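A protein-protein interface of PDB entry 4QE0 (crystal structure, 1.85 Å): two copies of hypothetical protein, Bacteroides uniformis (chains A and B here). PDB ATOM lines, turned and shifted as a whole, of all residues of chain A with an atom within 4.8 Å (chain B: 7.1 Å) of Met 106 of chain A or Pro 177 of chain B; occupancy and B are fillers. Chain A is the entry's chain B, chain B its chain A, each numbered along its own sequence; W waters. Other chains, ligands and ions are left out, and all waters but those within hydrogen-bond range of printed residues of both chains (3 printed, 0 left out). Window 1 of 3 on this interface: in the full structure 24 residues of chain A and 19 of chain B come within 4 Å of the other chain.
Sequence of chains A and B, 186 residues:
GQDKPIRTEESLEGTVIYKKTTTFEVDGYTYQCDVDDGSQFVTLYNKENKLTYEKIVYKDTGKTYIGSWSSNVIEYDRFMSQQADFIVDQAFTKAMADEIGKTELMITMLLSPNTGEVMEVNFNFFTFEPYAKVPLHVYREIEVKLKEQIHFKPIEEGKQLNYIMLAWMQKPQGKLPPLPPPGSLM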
ATOM      1  N   GLU A 104     -13.870  -2.841  -7.808  1.00  0.00           N
ATOM      2  CA  GLU A 104     -13.663  -4.146  -7.180  1.00  0.00           C
ATOM      3  C   GLU A 104     -13.766  -5.316  -8.155  1.00  0.00           C
ATOM      4  O   GLU A 104     -14.526  -5.269  -9.121  1.00  0.00           O
ATOM      5  CB  GLU A 104     -14.654  -4.318  -6.040  1.00  0.00           C
ATOM      6  CG  GLU A 104     -14.470  -3.275  -4.956  1.00  0.00           C
ATOM      7  CD  GLU A 104     -15.378  -3.498  -3.760  1.00  0.00           C
ATOM      8  OE1 GLU A 104     -16.591  -3.666  -3.968  1.00  0.00           O
ATOM      9  OE2 GLU A 104     -14.877  -3.496  -2.620  1.00  0.00           O
ATOM     10  N   LEU A 105     -12.966  -6.343  -7.884  1.00  0.00           N
ATOM     11  CA  LEU A 105     -12.939  -7.603  -8.644  1.00  0.00           C
ATOM     12  C   LEU A 105     -13.923  -8.554  -7.979  1.00  0.00           C
ATOM     13  O   LEU A 105     -14.035  -8.536  -6.759  1.00  0.00           O
ATOM     14  CB  LEU A 105     -11.530  -8.199  -8.532  1.00  0.00           C
ATOM     15  CG  LEU A 105     -11.252  -9.590  -9.091  1.00  0.00           C
ATOM     16  CD1 LEU A 105     -11.470  -9.582 -10.598  1.00  0.00           C
ATOM     17  CD2 LEU A 105      -9.821  -9.995  -8.783  1.00  0.00           C
ATOM     18  N   MET A 106     -14.635  -9.371  -8.755  1.00  0.00           N
ATOM     19  CA  MET A 106     -15.390 -10.452  -8.146  1.00  0.00           C
ATOM     20  C   MET A 106     -14.593 -11.722  -8.217  1.00  0.00           C
ATOM     21  O   MET A 106     -14.088 -12.097  -9.297  1.00  0.00           O
ATOM     22  CB  MET A 106     -16.723 -10.710  -8.854  1.00  0.00           C
ATOM     23  CG  MET A 106     -17.480 -11.778  -8.073  1.00  0.00           C
ATOM     24  SD  MET A 106     -19.381 -11.623  -8.639  1.00  0.00           S
ATOM     25  CE  MET A 106     -19.524 -13.128  -9.851  1.00  0.00           C
ATOM     26  N   ILE A 107     -14.452 -12.381  -7.075  1.00  0.00           N
ATOM     27  CA  ILE A 107     -13.773 -13.673  -6.999  1.00  0.00           C
ATOM     28  C   ILE A 107     -14.803 -14.678  -6.525  1.00  0.00           C
ATOM     29  O   ILE A 107     -15.560 -14.413  -5.561  1.00  0.00           O
ATOM     30  CB  ILE A 107     -12.580 -13.665  -6.007  1.00  0.00           C
ATOM     31  CG1 ILE A 107     -11.610 -12.507  -6.289  1.00  0.00           C
ATOM     32  CG2 ILE A 107     -11.826 -14.990  -6.066  1.00  0.00           C
ATOM     33  CD1 ILE A 107     -11.863 -11.263  -5.451  1.00  0.00           C
ATOM     34  N   THR A 108     -14.854 -15.824  -7.195  1.00  0.00           N
ATOM     35  CA  THR A 108     -15.748 -16.906  -6.792  1.00  0.00           C
ATOM     36  C   THR A 108     -14.958 -18.193  -6.541  1.00  0.00           C
ATOM     37  O   THR A 108     -14.150 -18.606  -7.381  1.00  0.00           O
ATOM     38  CB  THR A 108     -16.793 -17.178  -7.890  1.00  0.00           C
ATOM     39  OG1 THR A 108     -17.542 -15.992  -8.110  1.00  0.00           O
ATOM     40  CG2 THR A 108     -17.724 -18.281  -7.489  1.00  0.00           C
ATOM     41  N   ASN A 122     -13.065 -18.774 -10.101  1.00  0.00           N
ATOM     42  CA  ASN A 122     -13.177 -17.960 -11.322  1.00  0.00           C
ATOM     43  C   ASN A 122     -13.298 -16.490 -10.964  1.00  0.00           C
ATOM     44  O   ASN A 122     -13.524 -16.145  -9.796  1.00  0.00           O
ATOM     45  CB  ASN A 122     -14.266 -18.485 -12.255  1.00  0.00           C
ATOM     46  CG  ASN A 122     -15.643 -18.433 -11.645  1.00  0.00           C
ATOM     47  OD1 ASN A 122     -16.138 -17.359 -11.328  1.00  0.00           O
ATOM     48  ND2 ASN A 122     -16.272 -19.590 -11.478  1.00  0.00           N
ATOM     49  N   PHE A 123     -13.110 -15.645 -11.972  1.00  0.00           N
ATOM     50  CA  PHE A 123     -13.054 -14.204 -11.791  1.00  0.00           C
ATOM     51  C   PHE A 123     -14.037 -13.518 -12.710  1.00  0.00           C
ATOM     52  O   PHE A 123     -14.274 -13.980 -13.848  1.00  0.00           O
ATOM     53  CB  PHE A 123     -11.647 -13.699 -12.103  1.00  0.00           C
ATOM     54  CG  PHE A 123     -10.582 -14.372 -11.283  1.00  0.00           C
ATOM     55  CD1 PHE A 123     -10.336 -13.970  -9.999  1.00  0.00           C
ATOM     56  CD2 PHE A 123      -9.859 -15.434 -11.806  1.00  0.00           C
ATOM     57  CE1 PHE A 123      -9.378 -14.604  -9.223  1.00  0.00           C
ATOM     58  CE2 PHE A 123      -8.886 -16.059 -11.043  1.00  0.00           C
ATOM     59  CZ  PHE A 123      -8.641 -15.646  -9.753  1.00  0.00           C
ATOM     60  N   ASN A 124     -14.608 -12.421 -12.223  1.00  0.00           N
ATOM     61  CA  ASN A 124     -15.503 -11.619 -13.056  1.00  0.00           C
ATOM     62  C   ASN A 124     -15.209 -10.144 -12.929  1.00  0.00           C
ATOM     63  O   ASN A 124     -14.891  -9.637 -11.841  1.00  0.00           O
ATOM     64  CB  ASN A 124     -16.974 -11.830 -12.678  1.00  0.00           C
ATOM     65  CG  ASN A 124     -17.472 -13.225 -12.967  1.00  0.00           C
ATOM     66  OD1 ASN A 124     -17.699 -13.988 -12.049  1.00  0.00           O
ATOM     67  ND2 ASN A 124     -17.701 -13.535 -14.219  1.00  0.00           N
ATOM     68  N   MET A 165     -20.974 -22.071  -3.162  1.00  0.00           N
ATOM     69  CA  MET A 165     -20.363 -20.924  -3.838  1.00  0.00           C
ATOM     70  C   MET A 165     -20.049 -19.886  -2.817  1.00  0.00           C
ATOM     71  O   MET A 165     -20.941 -19.421  -2.102  1.00  0.00           O
ATOM     72  CB  MET A 165     -21.331 -20.349  -4.873  1.00  0.00           C
ATOM     73  CG  MET A 165     -20.667 -19.172  -5.577  1.00  0.00           C
ATOM     74  SD  MET A 165     -21.921 -18.417  -6.905  1.00  0.00           S
ATOM     75  CE  MET A 165     -21.873 -19.816  -8.287  1.00  0.00           C
ATOM     76  N   ALA A 167     -18.622 -16.229  -3.082  1.00  0.00           N
ATOM     77  CA  ALA A 167     -18.270 -15.159  -4.026  1.00  0.00           C
ATOM     78  C   ALA A 167     -18.163 -13.879  -3.228  1.00  0.00           C
ATOM     79  O   ALA A 167     -18.990 -13.640  -2.348  1.00  0.00           O
ATOM     80  CB  ALA A 167     -19.346 -15.029  -5.086  1.00  0.00           C
ATOM     81  N   TRP A 168     -17.165 -13.058  -3.537  1.00  0.00           N
ATOM     82  CA  TRP A 168     -17.017 -11.762  -2.894  1.00  0.00           C
ATOM     83  C   TRP A 168     -16.360 -10.753  -3.808  1.00  0.00           C
ATOM     84  O   TRP A 168     -15.750 -11.108  -4.829  1.00  0.00           O
ATOM     85  CB  TRP A 168     -16.261 -11.882  -1.573  1.00  0.00           C
ATOM     86  CG  TRP A 168     -14.785 -12.067  -1.642  1.00  0.00           C
ATOM     87  CD1 TRP A 168     -13.822 -11.120  -1.403  1.00  0.00           C
ATOM     88  CD2 TRP A 168     -14.085 -13.270  -1.973  1.00  0.00           C
ATOM     89  NE1 TRP A 168     -12.573 -11.657  -1.541  1.00  0.00           N
ATOM     90  CE2 TRP A 168     -12.698 -12.980  -1.873  1.00  0.00           C
ATOM     91  CE3 TRP A 168     -14.490 -14.564  -2.306  1.00  0.00           C
ATOM     92  CZ2 TRP A 168     -11.723 -13.921  -2.126  1.00  0.00           C
ATOM     93  CZ3 TRP A 168     -13.513 -15.517  -2.570  1.00  0.00           C
ATOM     94  CH2 TRP A 168     -12.144 -15.185  -2.482  1.00  0.00           C
ATOM     95  N   MET A 169     -16.536  -9.491  -3.442  1.00  0.00           N
ATOM     96  CA  MET A 169     -15.969  -8.359  -4.166  1.00  0.00           C
ATOM     97  C   MET A 169     -14.820  -7.849  -3.368  1.00  0.00           C
ATOM     98  O   MET A 169     -14.910  -7.714  -2.146  1.00  0.00           O
ATOM     99  CB  MET A 169     -16.951  -7.191  -4.260  1.00  0.00           C
ATOM    100  CG  MET A 169     -18.348  -7.532  -4.729  1.00  0.00           C
ATOM    101  SD  MET A 169     -18.361  -8.052  -6.608  1.00  0.00           S
ATOM    102  CE  MET A 169     -17.287  -6.628  -7.452  1.00  0.00           C
ATOM    103  N   ARG B  78     -31.631 -11.241 -19.211  1.00  0.00           N
ATOM    104  CA  ARG B  78     -31.637 -11.931 -17.944  1.00  0.00           C
ATOM    105  C   ARG B  78     -30.476 -11.473 -17.067  1.00  0.00           C
ATOM    106  O   ARG B  78     -30.663 -11.052 -15.924  1.00  0.00           O
ATOM    107  CB  ARG B  78     -31.569 -13.451 -18.175  1.00  0.00           C
ATOM    108  CG  ARG B  78     -31.808 -14.292 -16.918  1.00  0.00           C
ATOM    109  CD  ARG B  78     -30.556 -14.610 -16.154  1.00  0.00           C
ATOM    110  NE  ARG B  78     -29.423 -15.072 -16.954  1.00  0.00           N
ATOM    111  CZ  ARG B  78     -28.186 -15.141 -16.474  1.00  0.00           C
ATOM    112  NH1 ARG B  78     -27.956 -14.822 -15.212  1.00  0.00           N
ATOM    113  NH2 ARG B  78     -27.167 -15.544 -17.239  1.00  0.00           N
ATOM    114  N   PHE B  79     -29.273 -11.524 -17.614  1.00  0.00           N
ATOM    115  CA  PHE B  79     -28.113 -11.146 -16.850  1.00  0.00           C
ATOM    116  C   PHE B  79     -28.168  -9.708 -16.350  1.00  0.00           C
ATOM    117  O   PHE B  79     -27.871  -9.443 -15.178  1.00  0.00           O
ATOM    118  CB  PHE B  79     -26.813 -11.363 -17.632  1.00  0.00           C
ATOM    119  CG  PHE B  79     -25.594 -10.927 -16.849  1.00  0.00           C
ATOM    120  CD1 PHE B  79     -25.242 -11.573 -15.689  1.00  0.00           C
ATOM    121  CD2 PHE B  79     -24.874  -9.805 -17.232  1.00  0.00           C
ATOM    122  CE1 PHE B  79     -24.155 -11.157 -14.935  1.00  0.00           C
ATOM    123  CE2 PHE B  79     -23.790  -9.367 -16.476  1.00  0.00           C
ATOM    124  CZ  PHE B  79     -23.432 -10.043 -15.332  1.00  0.00           C
ATOM    125  N   GLN B  82     -30.641  -9.317 -13.496  1.00  0.00           N
ATOM    126  CA  GLN B  82     -30.194  -9.914 -12.253  1.00  0.00           C
ATOM    127  C   GLN B  82     -29.006  -9.172 -11.709  1.00  0.00           C
ATOM    128  O   GLN B  82     -28.823  -9.084 -10.488  1.00  0.00           O
ATOM    129  CB  GLN B  82     -29.879 -11.389 -12.444  1.00  0.00           C
ATOM    130  CG  GLN B  82     -31.130 -12.201 -12.747  1.00  0.00           C
ATOM    131  CD  GLN B  82     -30.857 -13.684 -12.880  1.00  0.00           C
ATOM    132  OE1 GLN B  82     -29.725 -14.099 -13.076  1.00  0.00           O
ATOM    133  NE2 GLN B  82     -31.910 -14.486 -12.815  1.00  0.00           N
ATOM    134  N   GLN B  83     -28.193  -8.612 -12.602  1.00  0.00           N
ATOM    135  CA  GLN B  83     -27.045  -7.832 -12.121  1.00  0.00           C
ATOM    136  C   GLN B  83     -27.495  -6.561 -11.395  1.00  0.00           C
ATOM    137  O   GLN B  83     -26.871  -6.176 -10.396  1.00  0.00           O
ATOM    138  CB  GLN B  83     -26.095  -7.537 -13.276  1.00  0.00           C
ATOM    139  CG  GLN B  83     -24.785  -6.852 -12.876  1.00  0.00           C
ATOM    140  CD  GLN B  83     -23.822  -7.708 -12.079  1.00  0.00           C
ATOM    141  OE1 GLN B  83     -24.044  -8.890 -11.824  1.00  0.00           O
ATOM    142  NE2 GLN B  83     -22.711  -7.084 -11.680  1.00  0.00           N
ATOM    143  N   PHE B  86     -28.482  -7.651  -8.041  1.00  0.00           N
ATOM    144  CA  PHE B  86     -27.275  -7.973  -7.294  1.00  0.00           C
ATOM    145  C   PHE B  86     -26.569  -6.709  -6.765  1.00  0.00           C
ATOM    146  O   PHE B  86     -26.108  -6.672  -5.626  1.00  0.00           O
ATOM    147  CB  PHE B  86     -26.324  -8.800  -8.141  1.00  0.00           C
ATOM    148  CG  PHE B  86     -25.062  -9.149  -7.412  1.00  0.00           C
ATOM    149  CD1 PHE B  86     -25.116  -9.992  -6.308  1.00  0.00           C
ATOM    150  CD2 PHE B  86     -23.855  -8.579  -7.764  1.00  0.00           C
ATOM    151  CE1 PHE B  86     -23.970 -10.309  -5.589  1.00  0.00           C
ATOM    152  CE2 PHE B  86     -22.698  -8.895  -7.051  1.00  0.00           C
ATOM    153  CZ  PHE B  86     -22.759  -9.760  -5.972  1.00  0.00           C
ATOM    154  N   GLY B 174     -28.761 -10.924   0.752  1.00  0.00           N
ATOM    155  CA  GLY B 174     -27.508 -11.693   0.696  1.00  0.00           C
ATOM    156  C   GLY B 174     -27.518 -12.754  -0.409  1.00  0.00           C
ATOM    157  O   GLY B 174     -26.987 -13.846  -0.261  1.00  0.00           O
ATOM    158  N   MLY B 175     -28.115 -12.409  -1.534  1.00  0.00           N
ATOM    159  CA  MLY B 175     -28.144 -13.273  -2.703  1.00  0.00           C
ATOM    160  CB  MLY B 175     -28.999 -12.682  -3.801  1.00  0.00           C
ATOM    161  CG  MLY B 175     -30.464 -12.596  -3.417  1.00  0.00           C
ATOM    162  CD  MLY B 175     -31.266 -12.055  -4.596  1.00  0.00           C
ATOM    163  CE  MLY B 175     -32.732 -11.819  -4.264  1.00  0.00           C
ATOM    164  NZ  MLY B 175     -33.358 -11.026  -5.365  1.00  0.00           N
ATOM    165  CH1 MLY B 175     -33.716 -11.931  -6.473  1.00  0.00           C
ATOM    166  CH2 MLY B 175     -34.560 -10.334  -4.888  1.00  0.00           C
ATOM    167  C   MLY B 175     -26.762 -13.472  -3.287  1.00  0.00           C
ATOM    168  O   MLY B 175     -25.900 -12.592  -3.210  1.00  0.00           O
ATOM    169  N   LEU B 176     -26.574 -14.647  -3.859  1.00  0.00           N
ATOM    170  CA  LEU B 176     -25.405 -14.933  -4.693  1.00  0.00           C
ATOM    171  C   LEU B 176     -25.454 -14.113  -5.962  1.00  0.00           C
ATOM    172  O   LEU B 176     -26.543 -13.712  -6.399  1.00  0.00           O
ATOM    173  CB  LEU B 176     -25.378 -16.413  -5.033  1.00  0.00           C
ATOM    174  CG  LEU B 176     -25.003 -17.296  -3.851  1.00  0.00           C
ATOM    175  CD1 LEU B 176     -25.278 -18.743  -4.205  1.00  0.00           C
ATOM    176  CD2 LEU B 176     -23.555 -17.091  -3.439  1.00  0.00           C
ATOM    177  N   PRO B 177     -24.290 -13.875  -6.583  1.00  0.00           N
ATOM    178  CA  PRO B 177     -24.312 -13.183  -7.861  1.00  0.00           C
ATOM    179  C   PRO B 177     -25.002 -13.994  -8.932  1.00  0.00           C
ATOM    180  O   PRO B 177     -25.132 -15.199  -8.801  1.00  0.00           O
ATOM    181  CB  PRO B 177     -22.835 -12.959  -8.197  1.00  0.00           C
ATOM    182  CG  PRO B 177     -22.070 -13.833  -7.304  1.00  0.00           C
ATOM    183  CD  PRO B 177     -22.926 -14.231  -6.154  1.00  0.00           C
ATOM    184  N   PRO B 178     -25.490 -13.326  -9.981  1.00  0.00           N
ATOM    185  CA  PRO B 178     -26.110 -14.071 -11.058  1.00  0.00           C
ATOM    186  C   PRO B 178     -25.129 -15.003 -11.776  1.00  0.00           C
ATOM    187  O   PRO B 178     -23.930 -14.732 -11.856  1.00  0.00           O
ATOM    188  CB  PRO B 178     -26.564 -13.007 -12.036  1.00  0.00           C
ATOM    189  CG  PRO B 178     -26.167 -11.697 -11.468  1.00  0.00           C
ATOM    190  CD  PRO B 178     -25.289 -11.905 -10.298  1.00  0.00           C
ATOM    191  N   LEU B 179     -25.676 -16.063 -12.346  1.00  0.00           N
ATOM    192  CA  LEU B 179     -24.938 -16.866 -13.308  1.00  0.00           C
ATOM    193  C   LEU B 179     -24.486 -15.949 -14.457  1.00  0.00           C
ATOM    194  O   LEU B 179     -25.258 -15.122 -14.967  1.00  0.00           O
ATOM    195  CB  LEU B 179     -25.852 -17.983 -13.837  1.00  0.00           C
ATOM    196  CG  LEU B 179     -25.219 -19.272 -14.340  1.00  0.00           C
ATOM    197  CD1 LEU B 179     -24.410 -19.944 -13.241  1.00  0.00           C
ATOM    198  CD2 LEU B 179     -26.320 -20.195 -14.843  1.00  0.00           C
ATOM    199  N   PRO B 180     -23.216 -16.054 -14.866  1.00  0.00           N
ATOM    200  CA  PRO B 180     -22.796 -15.172 -15.943  1.00  0.00           C
ATOM    201  C   PRO B 180     -23.503 -15.513 -17.259  1.00  0.00           C
ATOM    202  O   PRO B 180     -23.976 -16.637 -17.430  1.00  0.00           O
ATOM    203  CB  PRO B 180     -21.281 -15.405 -16.042  1.00  0.00           C
ATOM    204  CG  PRO B 180     -21.009 -16.648 -15.295  1.00  0.00           C
ATOM    205  CD  PRO B 180     -22.139 -16.907 -14.355  1.00  0.00           C
HETATM  206  O   HOH W   1     -22.032 -10.451 -11.032  1.00  0.00           O
HETATM  207  O   HOH W   2     -20.065  -8.480 -10.541  1.00  0.00           O
HETATM  208  O   HOH W   3     -25.043 -18.312  -9.025  1.00  0.00           O
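No position is printed for both chains.
Of the 3 pairs that touch across the chains among the printed residues, none has its exchanged pair printed and touching as well.
Among the printed residues, 3 pairs touch across the chains.
Among the printed residues, no Asp or Glu carboxylate lies within 4 Å of a Lys or Arg side-chain nitrogen of the other chain.
Among the printed residues, pairs that only touch across the chains: Met 106 of chain A with Pro 177 of chain B, Met 165 of chain A with Leu 176 of chain B and Ala 167 of chain A with Pro 177 of chain B.
Met 106 of chain A touches just one residue of chain B: Pro 177 (3.7 Å).
Pro 177 of chain B touches two residues of chain A.
Printed residues of chain B within 4 Å of Met 165 of chain A: Leu 176.
Printed residues of chain B within 4 Å of Ala 167 of chain A: Pro 177.
Printed residues of chain A within 4 Å of Leu 176 of chain B: Met 165 (3.7 Å).
The nearest residue of chain B that does not touch Met 106 of chain A is Phe 86 of chain B (4.6 Å).
Water W1 lies within hydrogen-bond range of the side-chain amide oxygen (OE1) of Gln 83 of chain B (2.7 Å) and the side-chain sulfur (SD) of Met 106 of chain A (3.8 Å).
Water W3 bridges O of Pro 177 of chain B (3.1 Å) and SD of Met 165 of chain A (3.8 Å).
Water W2 lies within hydrogen-bond range of NE2 of Gln 83 of chain B (3.2 Å) and SD of Met 106 of chain A (3.7 Å).
O of Met 106 of chain A lies within hydrogen-bond range of N of Asn 124 of chain A (3.0 Å).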
